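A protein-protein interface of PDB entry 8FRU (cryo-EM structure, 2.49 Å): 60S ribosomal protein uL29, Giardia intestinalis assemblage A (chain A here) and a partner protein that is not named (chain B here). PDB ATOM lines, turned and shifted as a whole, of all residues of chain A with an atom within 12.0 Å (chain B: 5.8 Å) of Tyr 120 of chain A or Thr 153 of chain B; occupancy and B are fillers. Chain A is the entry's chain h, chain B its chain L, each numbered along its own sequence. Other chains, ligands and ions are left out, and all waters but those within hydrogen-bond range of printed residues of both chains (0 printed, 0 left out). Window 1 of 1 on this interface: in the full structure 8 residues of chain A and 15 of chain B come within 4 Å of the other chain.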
ATOM      1  N   PHE A 115      34.277  -4.852   7.490  1.00  0.00           N
ATOM      2  CA  PHE A 115      33.292  -5.428   8.403  1.00  0.00           C
ATOM      3  C   PHE A 115      33.873  -5.442   9.806  1.00  0.00           C
ATOM      4  O   PHE A 115      34.257  -6.496  10.326  1.00  0.00           O
ATOM      5  CB  PHE A 115      32.878  -6.830   7.956  1.00  0.00           C
ATOM      6  CG  PHE A 115      32.221  -6.859   6.615  1.00  0.00           C
ATOM      7  CD1 PHE A 115      30.978  -6.290   6.432  1.00  0.00           C
ATOM      8  CD2 PHE A 115      32.850  -7.442   5.531  1.00  0.00           C
ATOM      9  CE1 PHE A 115      30.374  -6.305   5.201  1.00  0.00           C
ATOM     10  CE2 PHE A 115      32.249  -7.459   4.296  1.00  0.00           C
ATOM     11  CZ  PHE A 115      31.010  -6.893   4.132  1.00  0.00           C
ATOM     12  N   PRO A 116      33.967  -4.281  10.443  1.00  0.00           N
ATOM     13  CA  PRO A 116      34.468  -4.221  11.817  1.00  0.00           C
ATOM     14  C   PRO A 116      33.427  -4.673  12.830  1.00  0.00           C
ATOM     15  O   PRO A 116      32.225  -4.699  12.568  1.00  0.00           O
ATOM     16  CB  PRO A 116      34.801  -2.737  12.000  1.00  0.00           C
ATOM     17  CG  PRO A 116      33.881  -2.037  11.078  1.00  0.00           C
ATOM     18  CD  PRO A 116      33.669  -2.945   9.900  1.00  0.00           C
ATOM     19  N   LYS A 117      33.922  -5.029  14.011  1.00  0.00           N
ATOM     20  CA  LYS A 117      33.052  -5.442  15.103  1.00  0.00           C
ATOM     21  C   LYS A 117      32.249  -4.262  15.632  1.00  0.00           C
ATOM     22  O   LYS A 117      32.771  -3.156  15.792  1.00  0.00           O
ATOM     23  CB  LYS A 117      33.879  -6.046  16.233  1.00  0.00           C
ATOM     24  CG  LYS A 117      34.655  -7.289  15.846  1.00  0.00           C
ATOM     25  CD  LYS A 117      35.433  -7.823  17.034  1.00  0.00           C
ATOM     26  CE  LYS A 117      34.493  -8.399  18.078  1.00  0.00           C
ATOM     27  NZ  LYS A 117      33.973  -7.344  18.992  1.00  0.00           N
ATOM     28  N   LEU A 118      30.975  -4.505  15.922  1.00  0.00           N
ATOM     29  CA  LEU A 118      30.091  -3.478  16.447  1.00  0.00           C
ATOM     30  C   LEU A 118      29.440  -3.961  17.733  1.00  0.00           C
ATOM     31  O   LEU A 118      29.357  -5.160  18.003  1.00  0.00           O
ATOM     32  CB  LEU A 118      29.003  -3.088  15.442  1.00  0.00           C
ATOM     33  CG  LEU A 118      29.357  -3.091  13.959  1.00  0.00           C
ATOM     34  CD1 LEU A 118      28.097  -3.012  13.130  1.00  0.00           C
ATOM     35  CD2 LEU A 118      30.282  -1.939  13.631  1.00  0.00           C
ATOM     36  N   LYS A 119      28.972  -3.004  18.523  1.00  0.00           N
ATOM     37  CA  LYS A 119      28.238  -3.280  19.746  1.00  0.00           C
ATOM     38  C   LYS A 119      26.742  -3.210  19.483  1.00  0.00           C
ATOM     39  O   LYS A 119      26.260  -2.292  18.816  1.00  0.00           O
ATOM     40  CB  LYS A 119      28.619  -2.289  20.842  1.00  0.00           C
ATOM     41  CG  LYS A 119      30.033  -2.446  21.326  1.00  0.00           C
ATOM     42  CD  LYS A 119      30.071  -2.671  22.812  1.00  0.00           C
ATOM     43  CE  LYS A 119      30.405  -1.396  23.551  1.00  0.00           C
ATOM     44  NZ  LYS A 119      31.135  -1.684  24.815  1.00  0.00           N
ATOM     45  N   TYR A 120      26.013  -4.188  20.010  1.00  0.00           N
ATOM     46  CA  TYR A 120      24.572  -4.239  19.835  1.00  0.00           C
ATOM     47  C   TYR A 120      23.964  -4.984  21.012  1.00  0.00           C
ATOM     48  O   TYR A 120      24.647  -5.716  21.729  1.00  0.00           O
ATOM     49  CB  TYR A 120      24.191  -4.915  18.514  1.00  0.00           C
ATOM     50  CG  TYR A 120      24.610  -6.358  18.438  1.00  0.00           C
ATOM     51  CD1 TYR A 120      25.883  -6.709  18.030  1.00  0.00           C
ATOM     52  CD2 TYR A 120      23.738  -7.371  18.789  1.00  0.00           C
ATOM     53  CE1 TYR A 120      26.271  -8.024  17.968  1.00  0.00           C
ATOM     54  CE2 TYR A 120      24.118  -8.684  18.732  1.00  0.00           C
ATOM     55  CZ  TYR A 120      25.386  -9.007  18.320  1.00  0.00           C
ATOM     56  OH  TYR A 120      25.770 -10.323  18.259  1.00  0.00           O
ATOM     57  N   ALA A 121      22.667  -4.781  21.205  1.00  0.00           N
ATOM     58  CA  ALA A 121      21.900  -5.502  22.206  1.00  0.00           C
ATOM     59  C   ALA A 121      20.634  -6.044  21.562  1.00  0.00           C
ATOM     60  O   ALA A 121      20.136  -5.489  20.581  1.00  0.00           O
ATOM     61  CB  ALA A 121      21.544  -4.612  23.399  1.00  0.00           C
ATOM     62  N   VAL A 122      20.119  -7.137  22.115  1.00  0.00           N
ATOM     63  CA  VAL A 122      18.911  -7.781  21.614  1.00  0.00           C
ATOM     64  C   VAL A 122      17.796  -7.553  22.621  1.00  0.00           C
ATOM     65  O   VAL A 122      17.940  -7.886  23.803  1.00  0.00           O
ATOM     66  CB  VAL A 122      19.126  -9.281  21.357  1.00  0.00           C
ATOM     67  CG1 VAL A 122      17.979  -9.836  20.539  1.00  0.00           C
ATOM     68  CG2 VAL A 122      20.442  -9.517  20.643  1.00  0.00           C
ATOM     69  N   LYS A 123      16.686  -6.994  22.148  1.00  0.00           N
ATOM     70  CA  LYS A 123      15.566  -6.605  22.997  1.00  0.00           C
ATOM     71  C   LYS A 123      15.929  -5.403  23.854  1.00  0.00           C
ATOM     72  O   LYS A 123      15.706  -4.262  23.454  1.00  0.00           O
ATOM     73  CB  LYS A 123      15.117  -7.764  23.882  1.00  0.00           C
ATOM     74  CG  LYS A 123      14.572  -8.941  23.108  1.00  0.00           C
ATOM     75  CD  LYS A 123      14.830 -10.238  23.840  1.00  0.00           C
ATOM     76  CE  LYS A 123      13.611 -10.658  24.641  1.00  0.00           C
ATOM     77  NZ  LYS A 123      13.241  -9.634  25.657  1.00  0.00           N
ATOM     78  N   PRO B  77      27.172  -5.344  25.819  1.00  0.00           N
ATOM     79  CA  PRO B  77      25.971  -6.137  26.089  1.00  0.00           C
ATOM     80  C   PRO B  77      25.583  -7.151  25.011  1.00  0.00           C
ATOM     81  O   PRO B  77      24.417  -7.521  24.938  1.00  0.00           O
ATOM     82  CB  PRO B  77      24.895  -5.067  26.189  1.00  0.00           C
ATOM     83  CG  PRO B  77      25.330  -4.046  25.191  1.00  0.00           C
ATOM     84  CD  PRO B  77      26.835  -4.125  25.069  1.00  0.00           C
ATOM     85  N   CYS B  78      26.525  -7.590  24.191  1.00  0.00           N
ATOM     86  CA  CYS B  78      26.196  -8.575  23.174  1.00  0.00           C
ATOM     87  C   CYS B  78      25.825  -9.906  23.827  1.00  0.00           C
ATOM     88  O   CYS B  78      26.466 -10.325  24.790  1.00  0.00           O
ATOM     89  CB  CYS B  78      27.368  -8.775  22.218  1.00  0.00           C
ATOM     90  SG  CYS B  78      28.035  -7.254  21.502  1.00  0.00           S
ATOM     91  N   PRO B  79      24.800 -10.587  23.331  1.00  0.00           N
ATOM     92  CA  PRO B  79      24.469 -11.908  23.871  1.00  0.00           C
ATOM     93  C   PRO B  79      25.526 -12.946  23.527  1.00  0.00           C
ATOM     94  O   PRO B  79      26.255 -12.827  22.541  1.00  0.00           O
ATOM     95  CB  PRO B  79      23.129 -12.235  23.206  1.00  0.00           C
ATOM     96  CG  PRO B  79      23.102 -11.397  21.992  1.00  0.00           C
ATOM     97  CD  PRO B  79      23.822 -10.141  22.330  1.00  0.00           C
ATOM     98  N   GLN B  81      25.071 -16.082  22.590  1.00  0.00           N
ATOM     99  CA  GLN B  81      24.709 -16.897  21.441  1.00  0.00           C
ATOM    100  C   GLN B  81      24.335 -16.037  20.241  1.00  0.00           C
ATOM    101  O   GLN B  81      24.038 -14.850  20.362  1.00  0.00           O
ATOM    102  CB  GLN B  81      23.549 -17.829  21.791  1.00  0.00           C
ATOM    103  CG  GLN B  81      23.645 -18.420  23.171  1.00  0.00           C
ATOM    104  CD  GLN B  81      24.229 -19.806  23.168  1.00  0.00           C
ATOM    105  OE1 GLN B  81      25.147 -20.099  22.414  1.00  0.00           O
ATOM    106  NE2 GLN B  81      23.698 -20.670  24.015  1.00  0.00           N
ATOM    107  N   LYS B  82      24.356 -16.661  19.070  1.00  0.00           N
ATOM    108  CA  LYS B  82      23.947 -16.041  17.821  1.00  0.00           C
ATOM    109  C   LYS B  82      22.566 -16.533  17.416  1.00  0.00           C
ATOM    110  O   LYS B  82      22.080 -17.553  17.901  1.00  0.00           O
ATOM    111  CB  LYS B  82      24.952 -16.346  16.713  1.00  0.00           C
ATOM    112  CG  LYS B  82      26.385 -16.127  17.122  1.00  0.00           C
ATOM    113  CD  LYS B  82      27.332 -16.338  15.967  1.00  0.00           C
ATOM    114  CE  LYS B  82      28.476 -15.339  16.017  1.00  0.00           C
ATOM    115  NZ  LYS B  82      28.727 -14.847  17.396  1.00  0.00           N
ATOM    116  N   GLN B 121      28.109  -9.381  11.089  1.00  0.00           N
ATOM    117  CA  GLN B 121      28.416  -8.205  11.890  1.00  0.00           C
ATOM    118  C   GLN B 121      27.403  -8.004  13.007  1.00  0.00           C
ATOM    119  O   GLN B 121      27.778  -7.643  14.127  1.00  0.00           O
ATOM    120  CB  GLN B 121      28.476  -6.974  10.997  1.00  0.00           C
ATOM    121  CG  GLN B 121      29.555  -5.994  11.378  1.00  0.00           C
ATOM    122  CD  GLN B 121      29.641  -4.842  10.411  1.00  0.00           C
ATOM    123  OE1 GLN B 121      28.894  -4.780   9.439  1.00  0.00           O
ATOM    124  NE2 GLN B 121      30.553  -3.919  10.670  1.00  0.00           N
ATOM    125  N   ILE B 122      26.119  -8.222  12.735  1.00  0.00           N
ATOM    126  CA  ILE B 122      25.086  -7.994  13.744  1.00  0.00           C
ATOM    127  C   ILE B 122      24.698  -9.284  14.473  1.00  0.00           C
ATOM    128  O   ILE B 122      23.625  -9.355  15.062  1.00  0.00           O
ATOM    129  CB  ILE B 122      23.851  -7.305  13.153  1.00  0.00           C
ATOM    130  CG1 ILE B 122      23.132  -8.234  12.178  1.00  0.00           C
ATOM    131  CG2 ILE B 122      24.241  -6.009  12.478  1.00  0.00           C
ATOM    132  CD1 ILE B 122      21.825  -7.680  11.682  1.00  0.00           C
ATOM    133  N   GLY B 123      25.553 -10.300  14.448  1.00  0.00           N
ATOM    134  CA  GLY B 123      25.323 -11.485  15.250  1.00  0.00           C
ATOM    135  C   GLY B 123      24.379 -12.513  14.672  1.00  0.00           C
ATOM    136  O   GLY B 123      23.579 -13.097  15.411  1.00  0.00           O
ATOM    137  N   ILE B 124      24.459 -12.769  13.371  1.00  0.00           N
ATOM    138  CA  ILE B 124      23.651 -13.781  12.702  1.00  0.00           C
ATOM    139  C   ILE B 124      24.593 -14.832  12.136  1.00  0.00           C
ATOM    140  O   ILE B 124      25.615 -14.489  11.532  1.00  0.00           O
ATOM    141  CB  ILE B 124      22.783 -13.167  11.589  1.00  0.00           C
ATOM    142  CG1 ILE B 124      21.725 -12.241  12.182  1.00  0.00           C
ATOM    143  CG2 ILE B 124      22.146 -14.242  10.750  1.00  0.00           C
ATOM    144  CD1 ILE B 124      21.041 -11.373  11.164  1.00  0.00           C
ATOM    145  N   TYR B 148      13.910 -11.041  14.363  1.00  0.00           N
ATOM    146  CA  TYR B 148      15.162 -10.691  15.021  1.00  0.00           C
ATOM    147  C   TYR B 148      15.576  -9.267  14.685  1.00  0.00           C
ATOM    148  O   TYR B 148      15.972  -8.504  15.572  1.00  0.00           O
ATOM    149  CB  TYR B 148      16.259 -11.671  14.628  1.00  0.00           C
ATOM    150  CG  TYR B 148      17.620 -11.319  15.174  1.00  0.00           C
ATOM    151  CD1 TYR B 148      17.970 -11.639  16.477  1.00  0.00           C
ATOM    152  CD2 TYR B 148      18.562 -10.681  14.385  1.00  0.00           C
ATOM    153  CE1 TYR B 148      19.212 -11.331  16.974  1.00  0.00           C
ATOM    154  CE2 TYR B 148      19.805 -10.371  14.874  1.00  0.00           C
ATOM    155  CZ  TYR B 148      20.126 -10.698  16.168  1.00  0.00           C
ATOM    156  OH  TYR B 148      21.370 -10.387  16.655  1.00  0.00           O
ATOM    157  N   LYS B 151      13.877  -6.751  16.674  1.00  0.00           N
ATOM    158  CA  LYS B 151      14.163  -6.710  18.106  1.00  0.00           C
ATOM    159  C   LYS B 151      15.607  -6.341  18.451  1.00  0.00           C
ATOM    160  O   LYS B 151      15.981  -6.412  19.623  1.00  0.00           O
ATOM    161  CB  LYS B 151      13.808  -8.052  18.747  1.00  0.00           C
ATOM    162  CG  LYS B 151      12.312  -8.285  18.859  1.00  0.00           C
ATOM    163  CD  LYS B 151      11.972  -9.362  19.868  1.00  0.00           C
ATOM    164  CE  LYS B 151      13.010 -10.466  19.890  1.00  0.00           C
ATOM    165  NZ  LYS B 151      12.505 -11.662  20.630  1.00  0.00           N
ATOM    166  N   VAL B 152      16.418  -5.928  17.482  1.00  0.00           N
ATOM    167  CA  VAL B 152      17.848  -5.715  17.691  1.00  0.00           C
ATOM    168  C   VAL B 152      18.154  -4.224  17.658  1.00  0.00           C
ATOM    169  O   VAL B 152      17.599  -3.482  16.841  1.00  0.00           O
ATOM    170  CB  VAL B 152      18.689  -6.472  16.642  1.00  0.00           C
ATOM    171  CG1 VAL B 152      18.485  -5.881  15.265  1.00  0.00           C
ATOM    172  CG2 VAL B 152      20.157  -6.450  17.017  1.00  0.00           C
ATOM    173  N   THR B 153      19.045  -3.790  18.550  1.00  0.00           N
ATOM    174  CA  THR B 153      19.422  -2.388  18.685  1.00  0.00           C
ATOM    175  C   THR B 153      20.936  -2.243  18.599  1.00  0.00           C
ATOM    176  O   THR B 153      21.676  -3.046  19.171  1.00  0.00           O
ATOM    177  CB  THR B 153      18.926  -1.810  20.011  1.00  0.00           C
ATOM    178  OG1 THR B 153      17.549  -1.438  19.881  1.00  0.00           O
ATOM    179  CG2 THR B 153      19.734  -0.589  20.387  1.00  0.00           C
ATOM    180  N   ILE B 154      21.389  -1.207  17.896  1.00  0.00           N
ATOM    181  CA  ILE B 154      22.806  -0.978  17.632  1.00  0.00           C
ATOM    182  C   ILE B 154      23.249   0.298  18.332  1.00  0.00           C
ATOM    183  O   ILE B 154      22.525   1.300  18.331  1.00  0.00           O
ATOM    184  CB  ILE B 154      23.093  -0.882  16.122  1.00  0.00           C
ATOM    185  CG1 ILE B 154      22.512  -2.087  15.391  1.00  0.00           C
ATOM    186  CG2 ILE B 154      24.583  -0.784  15.873  1.00  0.00           C
ATOM    187  CD1 ILE B 154      22.945  -2.183  13.958  1.00  0.00           C
ATOM    188  N   PHE B 155      24.440   0.261  18.923  1.00  0.00           N
ATOM    189  CA  PHE B 155      25.026   1.407  19.607  1.00  0.00           C
ATOM    190  C   PHE B 155      26.200   1.939  18.803  1.00  0.00           C
ATOM    191  O   PHE B 155      27.076   1.173  18.391  1.00  0.00           O
ATOM    192  CB  PHE B 155      25.497   1.039  21.014  1.00  0.00           C
ATOM    193  CG  PHE B 155      24.414   0.516  21.892  1.00  0.00           C
ATOM    194  CD1 PHE B 155      23.444   1.360  22.387  1.00  0.00           C
ATOM    195  CD2 PHE B 155      24.368  -0.822  22.228  1.00  0.00           C
ATOM    196  CE1 PHE B 155      22.444   0.878  23.199  1.00  0.00           C
ATOM    197  CE2 PHE B 155      23.372  -1.309  23.038  1.00  0.00           C
ATOM    198  CZ  PHE B 155      22.407  -0.459  23.524  1.00  0.00           C
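Of the printed residues of chain B, Pro 116 of chain A touches Gln 121 (2.6 Å).
Printed residues of chain B within 4 Å of Lys 119 of chain A: Ile 154 (3.7 Å) and Phe 155 (3.1 Å).
Tyr 120 of chain A touches seven residues of chain B.
Printed residues of chain B within 4 Å of Val 122 of chain A: Pro 79 (3.5 Å) and Lys 151 (3.7 Å).
Of chain A, only Tyr 120 comes within 4 Å of Pro 77 of chain B.
Of chain A, only Tyr 120 comes within 4 Å of Cys 78 of chain B.
Pro 79 of chain B touches two residues of chain A.
Lys 82 of chain B touches none of the printed residues of chain A.
Of the printed residues of chain A, Gln 121 of chain B touches Phe 115 (3.8 Å), Pro 116 (2.6 Å) and Leu 118 (3.6 Å).
Of chain A, only Tyr 120 (3.7 Å) comes within 4 Å of Ile 122 of chain B.
Gly 123 of chain B touches one residue of chain A.
Ile 124 of chain B touches none of the printed residues of chain A.
Of chain A, only Ala 121 (3.7 Å) comes within 4 Å of Val 152 of chain B.
Thr 153 of chain B touches two residues of chain A.
Of chain A, only Lys 119 comes within 4 Å of Ile 154 of chain B.
Phe 155 of chain B touches just these residues of chain A: Lys 119 (3.1 Å) and Ala 121 (3.8 Å).
The nearest residue of chain B that does not touch Tyr 120 of chain A is Val 152 of chain B (4.1 Å).
The nearest residue of chain A that does not touch Thr 153 of chain B is Lys 119 of chain A (4.7 Å).
The backbone NH of Ala 121 of chain A is in hydrogen-bond range of the backbone carbonyl oxygen of Thr 153 of chain B.
The backbone carbonyl oxygen (O) of Lys 119 of chain A sits at hydrogen-bond distance from the backbone NH (N) of Phe 155 of chain B.
O of Tyr 120 of chain A lies close to SG of Cys 78 of chain B, at 3.7 Å.
O of Lys 151 of chain B sits at hydrogen-bond distance from N of Lys 123 of chain A, at 2.7 Å.
NE2 of Gln 121 of chain B is in hydrogen-bond range of O of Pro 116 of chain A (2.6 Å).
Among the printed residues, pairs that only touch across the chains: Phe 115 of chain A with Gln 121 of chain B (3.8 Å), Leu 118 of chain A with Gln 121 of chain B (3.6 Å), Lys 119 of chain A with Ile 154 of chain B (3.7 Å), Tyr 120 of chain A with Pro 77 of chain B (3.7 Å), Tyr 120 of chain A with Pro 79 of chain B (3.9 Å), Tyr 120 of chain A with Ile 122 of chain B (3.7 Å), Tyr 120 of chain A with Gly 123 of chain B (3.3 Å), Tyr 120 of chain A with Tyr 148 of chain B (3.8 Å), Tyr 120 of chain A with Thr 153 of chain B (3.2 Å), Ala 121 of chain A with Val 152 of chain B (3.7 Å), Ala 121 of chain A with Phe 155 of chain B (3.8 Å), Val 122 of chain A with Pro 79 of chain B (3.5 Å) and Val 122 of chain A with Lys 151 of chain B (3.7 Å).
The backbone carbonyl oxygen of Ile 122 of chain B is in hydrogen-bond range of the side-chain hydroxyl of Tyr 148 of chain B (2.9 Å).
Of the 9 printed residues of chain A, 8 touch a printed residue of chain B.
Of the 15 printed residues of chain B, 12 touch a printed residue of chain A.
Printed residues of chain B that touch a printed residue of chain A: Pro 77, Cys 78, Pro 79, Gln 121, Ile 122, Gly 123, Tyr 148, Lys 151, Val 152, Thr 153, Ile 154 and Phe 155.
Hydrophobic or aromatic side chains of chain B that line the printed part of chain A: Pro 77, Pro 79, Tyr 148, Val 152, Ile 154 and Phe 155.
Among the printed residues, 18 pairs touch across the chains.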
